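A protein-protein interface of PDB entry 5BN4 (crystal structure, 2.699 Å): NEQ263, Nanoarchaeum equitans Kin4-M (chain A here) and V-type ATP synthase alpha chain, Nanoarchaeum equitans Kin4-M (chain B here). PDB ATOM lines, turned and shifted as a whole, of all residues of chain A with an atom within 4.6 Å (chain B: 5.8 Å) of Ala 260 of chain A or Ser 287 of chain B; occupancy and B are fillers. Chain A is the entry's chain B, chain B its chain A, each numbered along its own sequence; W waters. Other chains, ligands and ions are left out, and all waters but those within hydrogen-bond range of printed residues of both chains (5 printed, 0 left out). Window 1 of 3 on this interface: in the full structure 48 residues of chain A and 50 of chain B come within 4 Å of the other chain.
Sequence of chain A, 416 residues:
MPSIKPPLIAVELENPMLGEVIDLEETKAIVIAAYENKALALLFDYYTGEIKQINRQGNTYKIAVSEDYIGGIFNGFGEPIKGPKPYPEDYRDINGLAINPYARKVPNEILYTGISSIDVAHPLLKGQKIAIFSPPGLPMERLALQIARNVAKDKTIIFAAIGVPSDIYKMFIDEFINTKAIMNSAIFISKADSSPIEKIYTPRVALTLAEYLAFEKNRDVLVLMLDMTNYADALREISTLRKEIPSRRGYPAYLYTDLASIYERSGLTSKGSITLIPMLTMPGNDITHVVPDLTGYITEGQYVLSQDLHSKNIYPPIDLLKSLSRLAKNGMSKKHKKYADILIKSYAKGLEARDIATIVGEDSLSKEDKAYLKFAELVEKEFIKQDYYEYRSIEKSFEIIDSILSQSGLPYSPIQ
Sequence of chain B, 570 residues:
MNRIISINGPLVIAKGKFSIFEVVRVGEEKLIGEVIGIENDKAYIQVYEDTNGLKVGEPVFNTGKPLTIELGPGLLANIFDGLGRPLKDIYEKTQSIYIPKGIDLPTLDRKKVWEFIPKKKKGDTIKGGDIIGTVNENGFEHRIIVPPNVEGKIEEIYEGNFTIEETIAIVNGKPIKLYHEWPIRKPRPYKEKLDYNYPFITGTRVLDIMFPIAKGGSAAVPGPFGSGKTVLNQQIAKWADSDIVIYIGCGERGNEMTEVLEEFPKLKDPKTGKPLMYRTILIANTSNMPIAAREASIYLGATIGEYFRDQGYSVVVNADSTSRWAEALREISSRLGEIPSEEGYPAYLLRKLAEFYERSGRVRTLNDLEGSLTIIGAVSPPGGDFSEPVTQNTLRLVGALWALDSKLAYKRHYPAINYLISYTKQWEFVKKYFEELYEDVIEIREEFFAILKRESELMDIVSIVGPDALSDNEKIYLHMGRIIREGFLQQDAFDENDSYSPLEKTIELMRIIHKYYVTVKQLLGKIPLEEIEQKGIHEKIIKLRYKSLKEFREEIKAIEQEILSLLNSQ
Tyr 256 of chain A touches Ser 287 of chain B (OH to CB, 3.7 Å).
Tyr 256 of chain A touches Arg 294 of chain B.
Thr 257 of chain A touches Ser 287 of chain B.
CB of Ala 260 of chain A touches OG of Ser 287 of chain B, 3.3 Å away.
Ala 260 of chain A touches Asn 288 of chain B.
Asn 288 of chain B touches Ser 261 of chain A (CB to CA, 3.7 Å).
Arg 253 of chain B touches Glu 264 of chain A.
Thr 286 of chain B touches Glu 264 of chain A.
Ser 287 of chain B touches Glu 264 of chain A.
Asn 288 of chain B touches Glu 264 of chain A.
Of the printed residues of chain B, Tyr 256 of chain A touches Gly 251, Glu 252, Ser 287 and Arg 294.
Printed residues of chain B within 4 Å of Thr 257 of chain A: Ser 287 (3.7 Å) and Arg 294 (2.8 Å).
Ile 262 of chain A touches none of the printed residues of chain B.
Of the printed residues of chain A, Arg 253 of chain B touches Glu 264 (3.7 Å) and Ile 298 (2.6 Å).
Of the printed residues of chain A, Thr 286 of chain B touches Glu 264 (3.9 Å).
Of chain A, only Tyr 256, Thr 257, Ala 260 and Glu 264 come within 4 Å of Ser 287 of chain B.
Met 289 of chain B touches none of the printed residues of chain A.
Printed residues of chain A within 4 Å of Arg 294 of chain B: Tyr 256 and Thr 257.
The nearest printed residue of chain A that does not touch Ser 287 of chain B is Ile 298 of chain A (4.9 Å).
The side-chain sulfur (SG) of Cys 250 of chain B lies within hydrogen-bond range of the backbone carbonyl oxygen (O) of Arg 294 of chain B, at 3.6 Å.
The backbone NH of Gly 251 of chain B is in hydrogen-bond range of the backbone carbonyl oxygen of Asn 285 of chain B (2.8 Å).
The backbone carbonyl oxygen of Glu 252 of chain B sits at hydrogen-bond distance from the backbone NH of Ser 287 of chain B, at 2.8 Å.
The backbone NH (N) of Gly 254 of chain B lies within hydrogen-bond range of the side-chain hydroxyl (OG1) of Thr 286 of chain B (3.2 Å).
The backbone NH (N) of Thr 286 of chain B sits at hydrogen-bond distance from the side-chain sulfur (SD) of Met 289 of chain B (3.5 Å).
The guanidinium group (NH2) of Arg 294 of chain B sits at hydrogen-bond distance from the backbone carbonyl oxygen (O) of Ser 287 of chain B.
Of the 10 printed residues of chain A, 6 touch a printed residue of chain B.
Of the 11 printed residues of chain B, 8 touch a printed residue of chain A.
Printed residues of chain B that touch a printed residue of chain A: Gly 251, Glu 252, Arg 253, Gly 254, Thr 286, Ser 287, Asn 288 and Arg 294.
Water W1 bridges the side-chain hydroxyl of Ser 287 of chain B (2.4 Å) and the side-chain carboxylate of Glu 264 of chain A (2.6 Å).
Water W3 lies within hydrogen-bond range of OE2 of Glu 264 of chain A (2.6 Å), OD1 of Asn 288 of chain B (2.6 Å) and OG1 of Thr 286 of chain B (3.4 Å).
Water W5 bridges the side-chain carboxylate of Glu 252 of chain B and the side-chain hydroxyl of Tyr 256 of chain A.
Water W2 bridges the backbone carbonyl oxygen of Glu 264 of chain A and the side-chain amide nitrogen of Asn 288 of chain B.
Water W4 bridges OE2 of Glu 264 of chain A (2.9 Å) and N of Gly 254 of chain B (3.4 Å).
O of Gly 251 of chain B sits at hydrogen-bond distance from OH of Tyr 256 of chain A (2.7 Å).
OE1 of Glu 252 of chain B sits at hydrogen-bond distance from OH of Tyr 256 of chain A, 3.4 Å away.
The guanidinium group (NE) of Arg 253 of chain B lies within hydrogen-bond range of the backbone carbonyl oxygen (O) of Ile 298 of chain A, 2.6 Å away.
The backbone NH (N) of Gly 254 of chain B is in hydrogen-bond range of the side-chain carboxylate (OE2) of Glu 264 of chain A (3.3 Å).
The side-chain hydroxyl (OG1) of Thr 257 of chain A sits at hydrogen-bond distance from the guanidinium group (NH2) of Arg 294 of chain B (2.8 Å).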
ATOM      1  N   TYR A 256     -23.383  31.404   7.508  1.00  0.00           N
ATOM      2  CA  TYR A 256     -23.261  30.810   8.838  1.00  0.00           C
ATOM      3  C   TYR A 256     -24.562  30.936   9.618  1.00  0.00           C
ATOM      4  O   TYR A 256     -25.075  29.956  10.161  1.00  0.00           O
ATOM      5  CB  TYR A 256     -22.128  31.477   9.623  1.00  0.00           C
ATOM      6  CG  TYR A 256     -22.043  31.058  11.079  1.00  0.00           C
ATOM      7  CD1 TYR A 256     -22.731  31.755  12.069  1.00  0.00           C
ATOM      8  CD2 TYR A 256     -21.268  29.972  11.464  1.00  0.00           C
ATOM      9  CE1 TYR A 256     -22.656  31.375  13.397  1.00  0.00           C
ATOM     10  CE2 TYR A 256     -21.183  29.587  12.790  1.00  0.00           C
ATOM     11  CZ  TYR A 256     -21.879  30.291  13.751  1.00  0.00           C
ATOM     12  OH  TYR A 256     -21.799  29.911  15.072  1.00  0.00           O
ATOM     13  N   THR A 257     -25.080  32.158   9.678  1.00  0.00           N
ATOM     14  CA  THR A 257     -26.273  32.460  10.454  1.00  0.00           C
ATOM     15  C   THR A 257     -27.492  31.732   9.904  1.00  0.00           C
ATOM     16  O   THR A 257     -28.321  31.223  10.662  1.00  0.00           O
ATOM     17  CB  THR A 257     -26.546  33.973  10.469  1.00  0.00           C
ATOM     18  OG1 THR A 257     -25.374  34.664  10.922  1.00  0.00           O
ATOM     19  CG2 THR A 257     -27.714  34.298  11.388  1.00  0.00           C
ATOM     20  N   ASP A 258     -27.596  31.687   8.581  1.00  0.00           N
ATOM     21  CA  ASP A 258     -28.706  31.008   7.926  1.00  0.00           C
ATOM     22  C   ASP A 258     -28.659  29.507   8.193  1.00  0.00           C
ATOM     23  O   ASP A 258     -29.683  28.887   8.482  1.00  0.00           O
ATOM     24  CB  ASP A 258     -28.688  31.274   6.422  1.00  0.00           C
ATOM     25  CG  ASP A 258     -29.835  30.603   5.700  1.00  0.00           C
ATOM     26  OD1 ASP A 258     -29.684  29.426   5.317  1.00  0.00           O
ATOM     27  OD2 ASP A 258     -30.887  31.251   5.520  1.00  0.00           O
ATOM     28  N   LEU A 259     -27.467  28.928   8.086  1.00  0.00           N
ATOM     29  CA  LEU A 259     -27.270  27.521   8.404  1.00  0.00           C
ATOM     30  C   LEU A 259     -27.567  27.278   9.876  1.00  0.00           C
ATOM     31  O   LEU A 259     -28.154  26.260  10.244  1.00  0.00           O
ATOM     32  CB  LEU A 259     -25.837  27.089   8.085  1.00  0.00           C
ATOM     33  CG  LEU A 259     -25.483  26.861   6.616  1.00  0.00           C
ATOM     34  CD1 LEU A 259     -23.982  26.690   6.454  1.00  0.00           C
ATOM     35  CD2 LEU A 259     -26.227  25.651   6.066  1.00  0.00           C
ATOM     36  N   ALA A 260     -27.160  28.223  10.716  1.00  0.00           N
ATOM     37  CA  ALA A 260     -27.399  28.122  12.148  1.00  0.00           C
ATOM     38  C   ALA A 260     -28.889  28.196  12.459  1.00  0.00           C
ATOM     39  O   ALA A 260     -29.358  27.602  13.427  1.00  0.00           O
ATOM     40  CB  ALA A 260     -26.649  29.209  12.887  1.00  0.00           C
ATOM     41  N   SER A 261     -29.633  28.916  11.623  1.00  0.00           N
ATOM     42  CA  SER A 261     -31.078  29.036  11.797  1.00  0.00           C
ATOM     43  C   SER A 261     -31.778  27.706  11.530  1.00  0.00           C
ATOM     44  O   SER A 261     -32.974  27.561  11.777  1.00  0.00           O
ATOM     45  CB  SER A 261     -31.643  30.112  10.869  1.00  0.00           C
ATOM     46  OG  SER A 261     -31.622  29.676   9.520  1.00  0.00           O
ATOM     47  N   ILE A 262     -31.021  26.740  11.023  1.00  0.00           N
ATOM     48  CA  ILE A 262     -31.546  25.415  10.726  1.00  0.00           C
ATOM     49  C   ILE A 262     -30.990  24.379  11.699  1.00  0.00           C
ATOM     50  O   ILE A 262     -31.742  23.606  12.291  1.00  0.00           O
ATOM     51  CB  ILE A 262     -31.211  25.004   9.280  1.00  0.00           C
ATOM     52  CG1 ILE A 262     -31.947  25.913   8.296  1.00  0.00           C
ATOM     53  CG2 ILE A 262     -31.568  23.546   9.026  1.00  0.00           C
ATOM     54  CD1 ILE A 262     -31.711  25.553   6.861  1.00  0.00           C
ATOM     55  N   TYR A 263     -29.673  24.377  11.868  1.00  0.00           N
ATOM     56  CA  TYR A 263     -29.015  23.395  12.723  1.00  0.00           C
ATOM     57  C   TYR A 263     -29.399  23.560  14.194  1.00  0.00           C
ATOM     58  O   TYR A 263     -29.453  22.583  14.937  1.00  0.00           O
ATOM     59  CB  TYR A 263     -27.495  23.478  12.570  1.00  0.00           C
ATOM     60  CG  TYR A 263     -26.981  23.191  11.174  1.00  0.00           C
ATOM     61  CD1 TYR A 263     -27.698  22.389  10.295  1.00  0.00           C
ATOM     62  CD2 TYR A 263     -25.775  23.724  10.738  1.00  0.00           C
ATOM     63  CE1 TYR A 263     -27.224  22.127   9.022  1.00  0.00           C
ATOM     64  CE2 TYR A 263     -25.297  23.468   9.469  1.00  0.00           C
ATOM     65  CZ  TYR A 263     -26.024  22.669   8.615  1.00  0.00           C
ATOM     66  OH  TYR A 263     -25.545  22.414   7.348  1.00  0.00           O
ATOM     67  N   GLU A 264     -29.666  24.795  14.608  1.00  0.00           N
ATOM     68  CA  GLU A 264     -30.014  25.073  16.000  1.00  0.00           C
ATOM     69  C   GLU A 264     -31.449  24.680  16.345  1.00  0.00           C
ATOM     70  O   GLU A 264     -31.803  24.573  17.520  1.00  0.00           O
ATOM     71  CB  GLU A 264     -29.770  26.544  16.342  1.00  0.00           C
ATOM     72  CG  GLU A 264     -28.304  26.907  16.502  1.00  0.00           C
ATOM     73  CD  GLU A 264     -27.679  26.270  17.730  1.00  0.00           C
ATOM     74  OE1 GLU A 264     -26.629  25.609  17.588  1.00  0.00           O
ATOM     75  OE2 GLU A 264     -28.235  26.433  18.836  1.00  0.00           O
ATOM     76  N   ILE A 298     -20.923  24.804  13.495  1.00  0.00           N
ATOM     77  CA  ILE A 298     -22.278  24.856  14.035  1.00  0.00           C
ATOM     78  C   ILE A 298     -22.729  23.527  14.644  1.00  0.00           C
ATOM     79  O   ILE A 298     -23.189  23.493  15.784  1.00  0.00           O
ATOM     80  CB  ILE A 298     -23.295  25.309  12.969  1.00  0.00           C
ATOM     81  CG1 ILE A 298     -22.849  26.633  12.344  1.00  0.00           C
ATOM     82  CG2 ILE A 298     -24.676  25.456  13.584  1.00  0.00           C
ATOM     83  CD1 ILE A 298     -23.723  27.106  11.203  1.00  0.00           C
ATOM     84  N   CYS B 250     -21.439  34.679  22.102  1.00  0.00           N
ATOM     85  CA  CYS B 250     -21.618  35.504  20.914  1.00  0.00           C
ATOM     86  C   CYS B 250     -21.767  34.659  19.652  1.00  0.00           C
ATOM     87  O   CYS B 250     -20.777  34.198  19.081  1.00  0.00           O
ATOM     88  CB  CYS B 250     -20.444  36.476  20.763  1.00  0.00           C
ATOM     89  SG  CYS B 250     -20.694  37.780  19.538  1.00  0.00           S
ATOM     90  N   GLY B 251     -23.010  34.456  19.228  1.00  0.00           N
ATOM     91  CA  GLY B 251     -23.301  33.769  17.982  1.00  0.00           C
ATOM     92  C   GLY B 251     -22.845  32.324  17.929  1.00  0.00           C
ATOM     93  O   GLY B 251     -22.399  31.852  16.884  1.00  0.00           O
ATOM     94  N   GLU B 252     -22.959  31.616  19.048  1.00  0.00           N
ATOM     95  CA  GLU B 252     -22.578  30.207  19.084  1.00  0.00           C
ATOM     96  C   GLU B 252     -23.739  29.304  19.494  1.00  0.00           C
ATOM     97  O   GLU B 252     -24.899  29.704  19.424  1.00  0.00           O
ATOM     98  CB  GLU B 252     -21.374  29.987  20.003  1.00  0.00           C
ATOM     99  CG  GLU B 252     -20.108  30.722  19.569  1.00  0.00           C
ATOM    100  CD  GLU B 252     -19.589  30.271  18.211  1.00  0.00           C
ATOM    101  OE1 GLU B 252     -19.923  29.148  17.786  1.00  0.00           O
ATOM    102  OE2 GLU B 252     -18.846  31.043  17.565  1.00  0.00           O
ATOM    103  N   ARG B 253     -23.417  28.085  19.915  1.00  0.00           N
ATOM    104  CA  ARG B 253     -24.432  27.080  20.228  1.00  0.00           C
ATOM    105  C   ARG B 253     -25.197  27.380  21.515  1.00  0.00           C
ATOM    106  O   ARG B 253     -24.624  27.856  22.496  1.00  0.00           O
ATOM    107  CB  ARG B 253     -23.799  25.688  20.315  1.00  0.00           C
ATOM    108  CG  ARG B 253     -23.142  25.221  19.026  1.00  0.00           C
ATOM    109  CD  ARG B 253     -22.484  23.859  19.202  1.00  0.00           C
ATOM    110  NE  ARG B 253     -21.776  23.438  17.997  1.00  0.00           N
ATOM    111  CZ  ARG B 253     -20.507  23.735  17.734  1.00  0.00           C
ATOM    112  NH1 ARG B 253     -19.799  24.455  18.593  1.00  0.00           N
ATOM    113  NH2 ARG B 253     -19.943  23.311  16.610  1.00  0.00           N
ATOM    114  N   GLY B 254     -26.495  27.086  21.507  1.00  0.00           N
ATOM    115  CA  GLY B 254     -27.335  27.281  22.675  1.00  0.00           C
ATOM    116  C   GLY B 254     -26.990  26.355  23.826  1.00  0.00           C
ATOM    117  O   GLY B 254     -26.928  26.785  24.980  1.00  0.00           O
ATOM    118  N   ASN B 285     -26.388  35.468  23.245  1.00  0.00           N
ATOM    119  CA  ASN B 285     -27.050  35.694  21.968  1.00  0.00           C
ATOM    120  C   ASN B 285     -26.569  34.656  20.965  1.00  0.00           C
ATOM    121  O   ASN B 285     -25.632  34.895  20.203  1.00  0.00           O
ATOM    122  CB  ASN B 285     -26.796  37.106  21.447  1.00  0.00           C
ATOM    123  CG  ASN B 285     -27.692  37.458  20.276  1.00  0.00           C
ATOM    124  OD1 ASN B 285     -28.842  37.852  20.460  1.00  0.00           O
ATOM    125  ND2 ASN B 285     -27.172  37.308  19.063  1.00  0.00           N
ATOM    126  N   THR B 286     -27.225  33.501  20.981  1.00  0.00           N
ATOM    127  CA  THR B 286     -26.791  32.337  20.221  1.00  0.00           C
ATOM    128  C   THR B 286     -26.791  32.576  18.708  1.00  0.00           C
ATOM    129  O   THR B 286     -27.249  33.614  18.229  1.00  0.00           O
ATOM    130  CB  THR B 286     -27.648  31.106  20.572  1.00  0.00           C
ATOM    131  OG1 THR B 286     -27.032  29.920  20.062  1.00  0.00           O
ATOM    132  CG2 THR B 286     -29.033  31.246  19.989  1.00  0.00           C
ATOM    133  N   SER B 287     -26.268  31.605  17.964  1.00  0.00           N
ATOM    134  CA  SER B 287     -26.054  31.759  16.526  1.00  0.00           C
ATOM    135  C   SER B 287     -27.327  32.067  15.741  1.00  0.00           C
ATOM    136  O   SER B 287     -27.303  32.868  14.807  1.00  0.00           O
ATOM    137  CB  SER B 287     -25.375  30.513  15.954  1.00  0.00           C
ATOM    138  OG  SER B 287     -26.199  29.369  16.104  1.00  0.00           O
ATOM    139  N   ASN B 288     -28.433  31.432  16.116  1.00  0.00           N
ATOM    140  CA  ASN B 288     -29.692  31.633  15.402  1.00  0.00           C
ATOM    141  C   ASN B 288     -30.603  32.676  16.046  1.00  0.00           C
ATOM    142  O   ASN B 288     -31.781  32.782  15.706  1.00  0.00           O
ATOM    143  CB  ASN B 288     -30.436  30.309  15.203  1.00  0.00           C
ATOM    144  CG  ASN B 288     -30.952  29.725  16.500  1.00  0.00           C
ATOM    145  OD1 ASN B 288     -30.332  29.872  17.550  1.00  0.00           O
ATOM    146  ND2 ASN B 288     -32.093  29.049  16.430  1.00  0.00           N
ATOM    147  N   MET B 289     -30.048  33.440  16.981  1.00  0.00           N
ATOM    148  CA  MET B 289     -30.737  34.599  17.535  1.00  0.00           C
ATOM    149  C   MET B 289     -30.376  35.806  16.665  1.00  0.00           C
ATOM    150  O   MET B 289     -29.459  35.701  15.848  1.00  0.00           O
ATOM    151  CB  MET B 289     -30.351  34.790  19.008  1.00  0.00           C
ATOM    152  CG  MET B 289     -31.207  33.957  19.958  1.00  0.00           C
ATOM    153  SD  MET B 289     -30.657  33.970  21.677  1.00  0.00           S
ATOM    154  CE  MET B 289     -31.049  35.654  22.146  1.00  0.00           C
ATOM    155  N   ARG B 294     -25.595  40.309  18.358  1.00  0.00           N
ATOM    156  CA  ARG B 294     -24.268  39.766  18.615  1.00  0.00           C
ATOM    157  C   ARG B 294     -23.335  40.908  18.989  1.00  0.00           C
ATOM    158  O   ARG B 294     -22.550  40.804  19.932  1.00  0.00           O
ATOM    159  CB  ARG B 294     -23.715  39.052  17.383  1.00  0.00           C
ATOM    160  CG  ARG B 294     -24.448  37.789  16.971  1.00  0.00           C
ATOM    161  CD  ARG B 294     -23.704  37.133  15.819  1.00  0.00           C
ATOM    162  NE  ARG B 294     -24.452  36.055  15.184  1.00  0.00           N
ATOM    163  CZ  ARG B 294     -24.022  35.386  14.118  1.00  0.00           C
ATOM    164  NH1 ARG B 294     -22.850  35.690  13.576  1.00  0.00           N
ATOM    165  NH2 ARG B 294     -24.760  34.418  13.593  1.00  0.00           N
HETATM  166  O   HOH W   1     -24.993  27.329  16.556  1.00  0.00           O
HETATM  167  O   HOH W   2     -33.350  26.761  18.353  1.00  0.00           O
HETATM  168  O   HOH W   3     -29.971  28.225  19.517  1.00  0.00           O
HETATM  169  O   HOH W   4     -28.020  24.209  20.633  1.00  0.00           O
HETATM  170  O   HOH W   5     -21.940  27.519  16.716  1.00  0.00           O
